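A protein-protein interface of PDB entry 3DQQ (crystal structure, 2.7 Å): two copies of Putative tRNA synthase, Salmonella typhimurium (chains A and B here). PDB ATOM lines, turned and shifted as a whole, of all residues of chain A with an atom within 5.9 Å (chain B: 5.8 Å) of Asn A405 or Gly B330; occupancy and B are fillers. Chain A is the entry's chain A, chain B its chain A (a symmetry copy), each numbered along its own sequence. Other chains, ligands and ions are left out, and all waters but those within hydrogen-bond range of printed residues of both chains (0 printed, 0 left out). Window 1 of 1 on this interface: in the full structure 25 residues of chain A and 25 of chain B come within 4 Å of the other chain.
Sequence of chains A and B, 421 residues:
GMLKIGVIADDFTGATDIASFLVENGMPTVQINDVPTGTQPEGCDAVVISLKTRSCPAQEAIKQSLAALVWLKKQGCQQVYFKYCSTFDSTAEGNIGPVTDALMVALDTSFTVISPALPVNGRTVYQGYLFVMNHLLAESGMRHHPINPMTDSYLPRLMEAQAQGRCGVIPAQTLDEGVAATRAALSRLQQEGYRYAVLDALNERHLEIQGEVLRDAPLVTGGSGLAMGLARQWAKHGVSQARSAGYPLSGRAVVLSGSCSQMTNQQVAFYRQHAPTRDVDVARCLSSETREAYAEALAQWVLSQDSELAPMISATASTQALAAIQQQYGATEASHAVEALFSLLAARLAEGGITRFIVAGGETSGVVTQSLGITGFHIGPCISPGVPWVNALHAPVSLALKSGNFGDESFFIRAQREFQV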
ATOM      1  N   SER A 259      28.019 -14.635 -35.406  1.00  0.00           N
ATOM      2  CA  SER A 259      27.486 -15.095 -34.134  1.00  0.00           C
ATOM      3  C   SER A 259      28.260 -14.611 -32.899  1.00  0.00           C
ATOM      4  O   SER A 259      29.500 -14.483 -32.877  1.00  0.00           O
ATOM      5  CB  SER A 259      27.410 -16.640 -34.135  1.00  0.00           C
ATOM      6  OG  SER A 259      27.001 -17.258 -32.897  1.00  0.00           O
ATOM      7  N   SER A 261      27.870 -16.231 -29.896  1.00  0.00           N
ATOM      8  CA  SER A 261      27.644 -17.315 -28.978  1.00  0.00           C
ATOM      9  C   SER A 261      28.892 -17.910 -28.329  1.00  0.00           C
ATOM     10  O   SER A 261      29.997 -17.699 -28.796  1.00  0.00           O
ATOM     11  CB  SER A 261      26.908 -18.421 -29.739  1.00  0.00           C
ATOM     12  OG  SER A 261      27.763 -19.124 -30.623  1.00  0.00           O
ATOM     13  N   GLN A 262      28.703 -18.697 -27.267  1.00  0.00           N
ATOM     14  CA  GLN A 262      29.809 -19.360 -26.584  1.00  0.00           C
ATOM     15  C   GLN A 262      30.587 -20.240 -27.521  1.00  0.00           C
ATOM     16  O   GLN A 262      31.817 -20.220 -27.528  1.00  0.00           O
ATOM     17  CB  GLN A 262      29.332 -20.151 -25.342  1.00  0.00           C
ATOM     18  CG  GLN A 262      29.404 -19.216 -24.042  1.00  0.00           C
ATOM     19  CD  GLN A 262      28.933 -19.844 -22.651  1.00  0.00           C
ATOM     20  OE1 GLN A 262      28.113 -20.804 -22.604  1.00  0.00           O
ATOM     21  NE2 GLN A 262      29.463 -19.276 -21.520  1.00  0.00           N
ATOM     22  N   MET A 263      29.883 -21.014 -28.334  1.00  0.00           N
ATOM     23  CA  MET A 263      30.578 -21.961 -29.178  1.00  0.00           C
ATOM     24  C   MET A 263      31.203 -21.245 -30.356  1.00  0.00           C
ATOM     25  O   MET A 263      32.317 -21.567 -30.744  1.00  0.00           O
ATOM     26  CB  MET A 263      29.667 -23.088 -29.634  1.00  0.00           C
ATOM     27  CG  MET A 263      30.412 -24.130 -30.468  1.00  0.00           C
ATOM     28  SD  MET A 263      31.647 -25.112 -29.562  1.00  0.00           S
ATOM     29  CE  MET A 263      33.089 -24.787 -30.486  1.00  0.00           C
ATOM     30  N   THR A 264      30.517 -20.266 -30.927  1.00  0.00           N
ATOM     31  CA  THR A 264      31.140 -19.525 -32.009  1.00  0.00           C
ATOM     32  C   THR A 264      32.428 -18.879 -31.480  1.00  0.00           C
ATOM     33  O   THR A 264      33.459 -18.864 -32.163  1.00  0.00           O
ATOM     34  CB  THR A 264      30.225 -18.457 -32.615  1.00  0.00           C
ATOM     35  OG1 THR A 264      28.930 -18.996 -32.836  1.00  0.00           O
ATOM     36  CG2 THR A 264      30.762 -17.981 -33.908  1.00  0.00           C
ATOM     37  N   LYS A 402      26.090 -22.261 -40.285  1.00  0.00           N
ATOM     38  CA  LYS A 402      26.105 -22.724 -38.930  1.00  0.00           C
ATOM     39  C   LYS A 402      25.380 -21.703 -38.072  1.00  0.00           C
ATOM     40  O   LYS A 402      25.619 -20.491 -38.135  1.00  0.00           O
ATOM     41  CB  LYS A 402      27.571 -22.814 -38.522  1.00  0.00           C
ATOM     42  CG  LYS A 402      27.903 -23.310 -37.141  1.00  0.00           C
ATOM     43  CD  LYS A 402      27.843 -22.204 -36.111  1.00  0.00           C
ATOM     44  CE  LYS A 402      29.008 -22.276 -35.181  1.00  0.00           C
ATOM     45  NZ  LYS A 402      28.683 -21.622 -33.896  1.00  0.00           N
ATOM     46  N   SER A 403      24.500 -22.212 -37.241  1.00  0.00           N
ATOM     47  CA  SER A 403      23.720 -21.408 -36.291  1.00  0.00           C
ATOM     48  C   SER A 403      24.295 -21.456 -34.829  1.00  0.00           C
ATOM     49  O   SER A 403      24.630 -22.549 -34.315  1.00  0.00           O
ATOM     50  CB  SER A 403      22.276 -21.972 -36.283  1.00  0.00           C
ATOM     51  OG  SER A 403      21.332 -20.929 -36.263  1.00  0.00           O
ATOM     52  N   GLY A 404      24.399 -20.287 -34.178  1.00  0.00           N
ATOM     53  CA  GLY A 404      24.576 -20.197 -32.713  1.00  0.00           C
ATOM     54  C   GLY A 404      25.567 -21.169 -32.088  1.00  0.00           C
ATOM     55  O   GLY A 404      26.760 -20.962 -32.216  1.00  0.00           O
ATOM     56  N   ASN A 405      25.070 -22.229 -31.430  1.00  0.00           N
ATOM     57  CA  ASN A 405      25.913 -23.223 -30.709  1.00  0.00           C
ATOM     58  C   ASN A 405      26.040 -24.628 -31.338  1.00  0.00           C
ATOM     59  O   ASN A 405      26.561 -25.545 -30.688  1.00  0.00           O
ATOM     60  CB  ASN A 405      25.495 -23.354 -29.223  1.00  0.00           C
ATOM     61  CG  ASN A 405      25.852 -22.082 -28.357  1.00  0.00           C
ATOM     62  OD1 ASN A 405      27.018 -21.615 -28.277  1.00  0.00           O
ATOM     63  ND2 ASN A 405      24.827 -21.556 -27.675  1.00  0.00           N
ATOM     64  N   PHE A 406      25.633 -24.787 -32.594  1.00  0.00           N
ATOM     65  CA  PHE A 406      26.030 -25.968 -33.381  1.00  0.00           C
ATOM     66  C   PHE A 406      27.532 -26.031 -33.677  1.00  0.00           C
ATOM     67  O   PHE A 406      28.207 -25.027 -33.839  1.00  0.00           O
ATOM     68  CB  PHE A 406      25.341 -26.011 -34.746  1.00  0.00           C
ATOM     69  CG  PHE A 406      23.876 -26.215 -34.675  1.00  0.00           C
ATOM     70  CD1 PHE A 406      23.340 -27.464 -34.879  1.00  0.00           C
ATOM     71  CD2 PHE A 406      23.013 -25.142 -34.389  1.00  0.00           C
ATOM     72  CE1 PHE A 406      21.973 -27.666 -34.816  1.00  0.00           C
ATOM     73  CE2 PHE A 406      21.631 -25.335 -34.300  1.00  0.00           C
ATOM     74  CZ  PHE A 406      21.114 -26.605 -34.529  1.00  0.00           C
ATOM     75  N   GLY A 407      28.010 -27.250 -33.818  1.00  0.00           N
ATOM     76  CA  GLY A 407      29.381 -27.516 -34.126  1.00  0.00           C
ATOM     77  C   GLY A 407      30.205 -27.738 -32.872  1.00  0.00           C
ATOM     78  O   GLY A 407      29.739 -27.555 -31.746  1.00  0.00           O
ATOM     79  N   THR B 319      21.126 -22.909 -16.164  1.00  0.00           N
ATOM     80  CA  THR B 319      21.264 -21.715 -17.027  1.00  0.00           C
ATOM     81  C   THR B 319      21.591 -22.024 -18.512  1.00  0.00           C
ATOM     82  O   THR B 319      21.340 -21.204 -19.402  1.00  0.00           O
ATOM     83  CB  THR B 319      22.353 -20.779 -16.409  1.00  0.00           C
ATOM     84  OG1 THR B 319      21.718 -19.624 -15.877  1.00  0.00           O
ATOM     85  CG2 THR B 319      23.469 -20.381 -17.421  1.00  0.00           C
ATOM     86  N   GLN B 320      22.141 -23.213 -18.764  1.00  0.00           N
ATOM     87  CA  GLN B 320      22.544 -23.652 -20.108  1.00  0.00           C
ATOM     88  C   GLN B 320      21.581 -24.693 -20.764  1.00  0.00           C
ATOM     89  O   GLN B 320      21.949 -25.360 -21.724  1.00  0.00           O
ATOM     90  CB  GLN B 320      23.997 -24.193 -20.002  1.00  0.00           C
ATOM     91  CG  GLN B 320      25.074 -23.105 -19.776  1.00  0.00           C
ATOM     92  CD  GLN B 320      25.388 -22.357 -21.074  1.00  0.00           C
ATOM     93  OE1 GLN B 320      24.670 -21.432 -21.481  1.00  0.00           O
ATOM     94  NE2 GLN B 320      26.439 -22.785 -21.749  1.00  0.00           N
ATOM     95  N   LEU B 322      18.144 -24.404 -22.167  1.00  0.00           N
ATOM     96  CA  LEU B 322      17.455 -24.035 -23.442  1.00  0.00           C
ATOM     97  C   LEU B 322      18.403 -24.258 -24.649  1.00  0.00           C
ATOM     98  O   LEU B 322      18.009 -24.898 -25.637  1.00  0.00           O
ATOM     99  CB  LEU B 322      16.962 -22.556 -23.436  1.00  0.00           C
ATOM    100  CG  LEU B 322      15.869 -22.063 -24.446  1.00  0.00           C
ATOM    101  CD1 LEU B 322      16.034 -20.562 -24.857  1.00  0.00           C
ATOM    102  CD2 LEU B 322      15.762 -22.951 -25.700  1.00  0.00           C
ATOM    103  N   ALA B 323      19.631 -23.716 -24.535  1.00  0.00           N
ATOM    104  CA  ALA B 323      20.771 -23.945 -25.447  1.00  0.00           C
ATOM    105  C   ALA B 323      21.157 -25.444 -25.748  1.00  0.00           C
ATOM    106  O   ALA B 323      21.631 -25.776 -26.851  1.00  0.00           O
ATOM    107  CB  ALA B 323      21.982 -23.201 -24.883  1.00  0.00           C
ATOM    108  N   GLN B 326      17.629 -26.709 -28.254  1.00  0.00           N
ATOM    109  CA  GLN B 326      17.785 -25.928 -29.498  1.00  0.00           C
ATOM    110  C   GLN B 326      19.067 -25.098 -29.405  1.00  0.00           C
ATOM    111  O   GLN B 326      19.145 -24.086 -28.684  1.00  0.00           O
ATOM    112  CB  GLN B 326      16.561 -25.069 -29.926  1.00  0.00           C
ATOM    113  CG  GLN B 326      15.541 -24.578 -28.878  1.00  0.00           C
ATOM    114  CD  GLN B 326      14.127 -25.123 -29.125  1.00  0.00           C
ATOM    115  OE1 GLN B 326      13.203 -24.387 -29.491  1.00  0.00           O
ATOM    116  NE2 GLN B 326      13.962 -26.420 -28.914  1.00  0.00           N
ATOM    117  N   GLN B 327      20.068 -25.549 -30.156  1.00  0.00           N
ATOM    118  CA  GLN B 327      21.429 -25.035 -30.044  1.00  0.00           C
ATOM    119  C   GLN B 327      21.648 -23.663 -30.698  1.00  0.00           C
ATOM    120  O   GLN B 327      22.739 -23.100 -30.591  1.00  0.00           O
ATOM    121  CB  GLN B 327      22.419 -26.048 -30.625  1.00  0.00           C
ATOM    122  CG  GLN B 327      22.130 -27.500 -30.235  1.00  0.00           C
ATOM    123  CD  GLN B 327      23.394 -28.332 -30.183  1.00  0.00           C
ATOM    124  OE1 GLN B 327      24.380 -28.039 -30.870  1.00  0.00           O
ATOM    125  NE2 GLN B 327      23.381 -29.370 -29.355  1.00  0.00           N
ATOM    126  N   GLN B 328      20.616 -23.150 -31.384  1.00  0.00           N
ATOM    127  CA  GLN B 328      20.556 -21.747 -31.868  1.00  0.00           C
ATOM    128  C   GLN B 328      20.548 -20.676 -30.749  1.00  0.00           C
ATOM    129  O   GLN B 328      21.013 -19.551 -30.969  1.00  0.00           O
ATOM    130  CB  GLN B 328      19.319 -21.553 -32.765  1.00  0.00           C
ATOM    131  CG  GLN B 328      17.954 -21.619 -32.019  1.00  0.00           C
ATOM    132  CD  GLN B 328      16.923 -22.491 -32.744  1.00  0.00           C
ATOM    133  OE1 GLN B 328      17.232 -23.614 -33.172  1.00  0.00           O
ATOM    134  NE2 GLN B 328      15.693 -21.981 -32.871  1.00  0.00           N
ATOM    135  N   TYR B 329      19.989 -21.032 -29.580  1.00  0.00           N
ATOM    136  CA  TYR B 329      19.999 -20.190 -28.358  1.00  0.00           C
ATOM    137  C   TYR B 329      21.309 -20.452 -27.599  1.00  0.00           C
ATOM    138  O   TYR B 329      21.990 -21.471 -27.845  1.00  0.00           O
ATOM    139  CB  TYR B 329      18.780 -20.489 -27.432  1.00  0.00           C
ATOM    140  CG  TYR B 329      17.447 -20.044 -28.001  1.00  0.00           C
ATOM    141  CD1 TYR B 329      16.910 -18.790 -27.675  1.00  0.00           C
ATOM    142  CD2 TYR B 329      16.734 -20.875 -28.897  1.00  0.00           C
ATOM    143  CE1 TYR B 329      15.681 -18.363 -28.224  1.00  0.00           C
ATOM    144  CE2 TYR B 329      15.506 -20.471 -29.456  1.00  0.00           C
ATOM    145  CZ  TYR B 329      14.987 -19.208 -29.120  1.00  0.00           C
ATOM    146  OH  TYR B 329      13.786 -18.802 -29.662  1.00  0.00           O
ATOM    147  N   GLY B 330      21.661 -19.525 -26.704  1.00  0.00           N
ATOM    148  CA  GLY B 330      22.756 -19.732 -25.773  1.00  0.00           C
ATOM    149  C   GLY B 330      22.214 -19.799 -24.357  1.00  0.00           C
ATOM    150  O   GLY B 330      21.187 -20.491 -24.055  1.00  0.00           O
ATOM    151  N   ALA B 331      22.915 -19.071 -23.486  1.00  0.00           N
ATOM    152  CA  ALA B 331      22.499 -18.869 -22.110  1.00  0.00           C
ATOM    153  C   ALA B 331      21.033 -18.371 -22.036  1.00  0.00           C
ATOM    154  O   ALA B 331      20.453 -17.889 -23.033  1.00  0.00           O
ATOM    155  CB  ALA B 331      23.446 -17.895 -21.415  1.00  0.00           C
ATOM    156  N   THR B 332      20.422 -18.587 -20.868  1.00  0.00           N
ATOM    157  CA  THR B 332      19.142 -17.973 -20.452  1.00  0.00           C
ATOM    158  C   THR B 332      19.380 -17.669 -18.953  1.00  0.00           C
ATOM    159  O   THR B 332      19.964 -18.514 -18.256  1.00  0.00           O
ATOM    160  CB  THR B 332      17.913 -18.926 -20.682  1.00  0.00           C
ATOM    161  OG1 THR B 332      17.840 -19.885 -19.620  1.00  0.00           O
ATOM    162  CG2 THR B 332      17.994 -19.661 -22.068  1.00  0.00           C
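OE1 of Gln A262 lies within hydrogen-bond range of NE2 of Gln B320.
N of Asn A405 is in hydrogen-bond range of O of Gln B327.
The backbone carbonyl oxygen of Tyr B329 lies within hydrogen-bond range of the side-chain amide nitrogen of Asn A405.
O of Gly A404 is in hydrogen-bond range of OG of Ser A261, 2.6 Å away.
The backbone NH (N) of Met A263 lies within hydrogen-bond range of the side-chain amide oxygen (OD1) of Asn A405, at 2.9 Å.
OG1 of Thr A264 lies within hydrogen-bond range of O of Gly A404, at 3.0 Å.
The side-chain amino group (NZ) of Lys A402 sits at hydrogen-bond distance from the backbone carbonyl oxygen (O) of Gly A404 (2.6 Å).
The side-chain amino group (NZ) of Lys A402 sits close to the backbone carbonyl oxygen (O) of Phe A406 (3.4 Å).
Among the printed residues, merely in contact across the chains: Gly A404 with Gln B327 (3.7 Å), Asn A405 with Gly B330 (3.4 Å), Phe A406 with Gln B327 (3.6 Å) and Phe A406 with Gln B328 (3.8 Å).
Asn A405 touches just these residues of chain B: Gln B327 (2.6 Å), Tyr B329 (2.8 Å) and Gly B330 (3.4 Å).
Gly B330 touches one residue of chain A.
Of the printed residues of chain A, Gln B327 touches Gly A404, Asn A405 and Phe A406.
Of the printed residues of chain B, Phe A406 touches Gln B327 (3.6 Å) and Gln B328 (3.8 Å).
Of the printed residues of chain B, Gly A404 touches Gln B327.
Of the printed residues of chain A, Gln B320 touches Gln A262.
Of the printed residues of chain A, Gln B328 touches Phe A406.
Thr B319 touches none of the printed residues of chain A.
The nearest printed residue of chain A that does not touch Gly B330 is Ser A261 (5.9 Å).
Of the 11 printed residues of chain B, 5 touch a printed residue of chain A.
Printed residues of chain B that touch a printed residue of chain A: Gln B320, Gln B327, Gln B328, Tyr B329 and Gly B330.
Along chain B the printed residues that touch a printed residue of chain A span positions 320 to 330.
Among the printed residues, 7 pairs touch across the chains.
Among the printed residues, no Asp or Glu carboxylate lies within 4 Å of a Lys or Arg side-chain nitrogen of the other chain.
No position is printed for both chains.
Of the 7 pairs that touch across the chains among the printed residues, none has its exchanged pair printed and touching as well.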
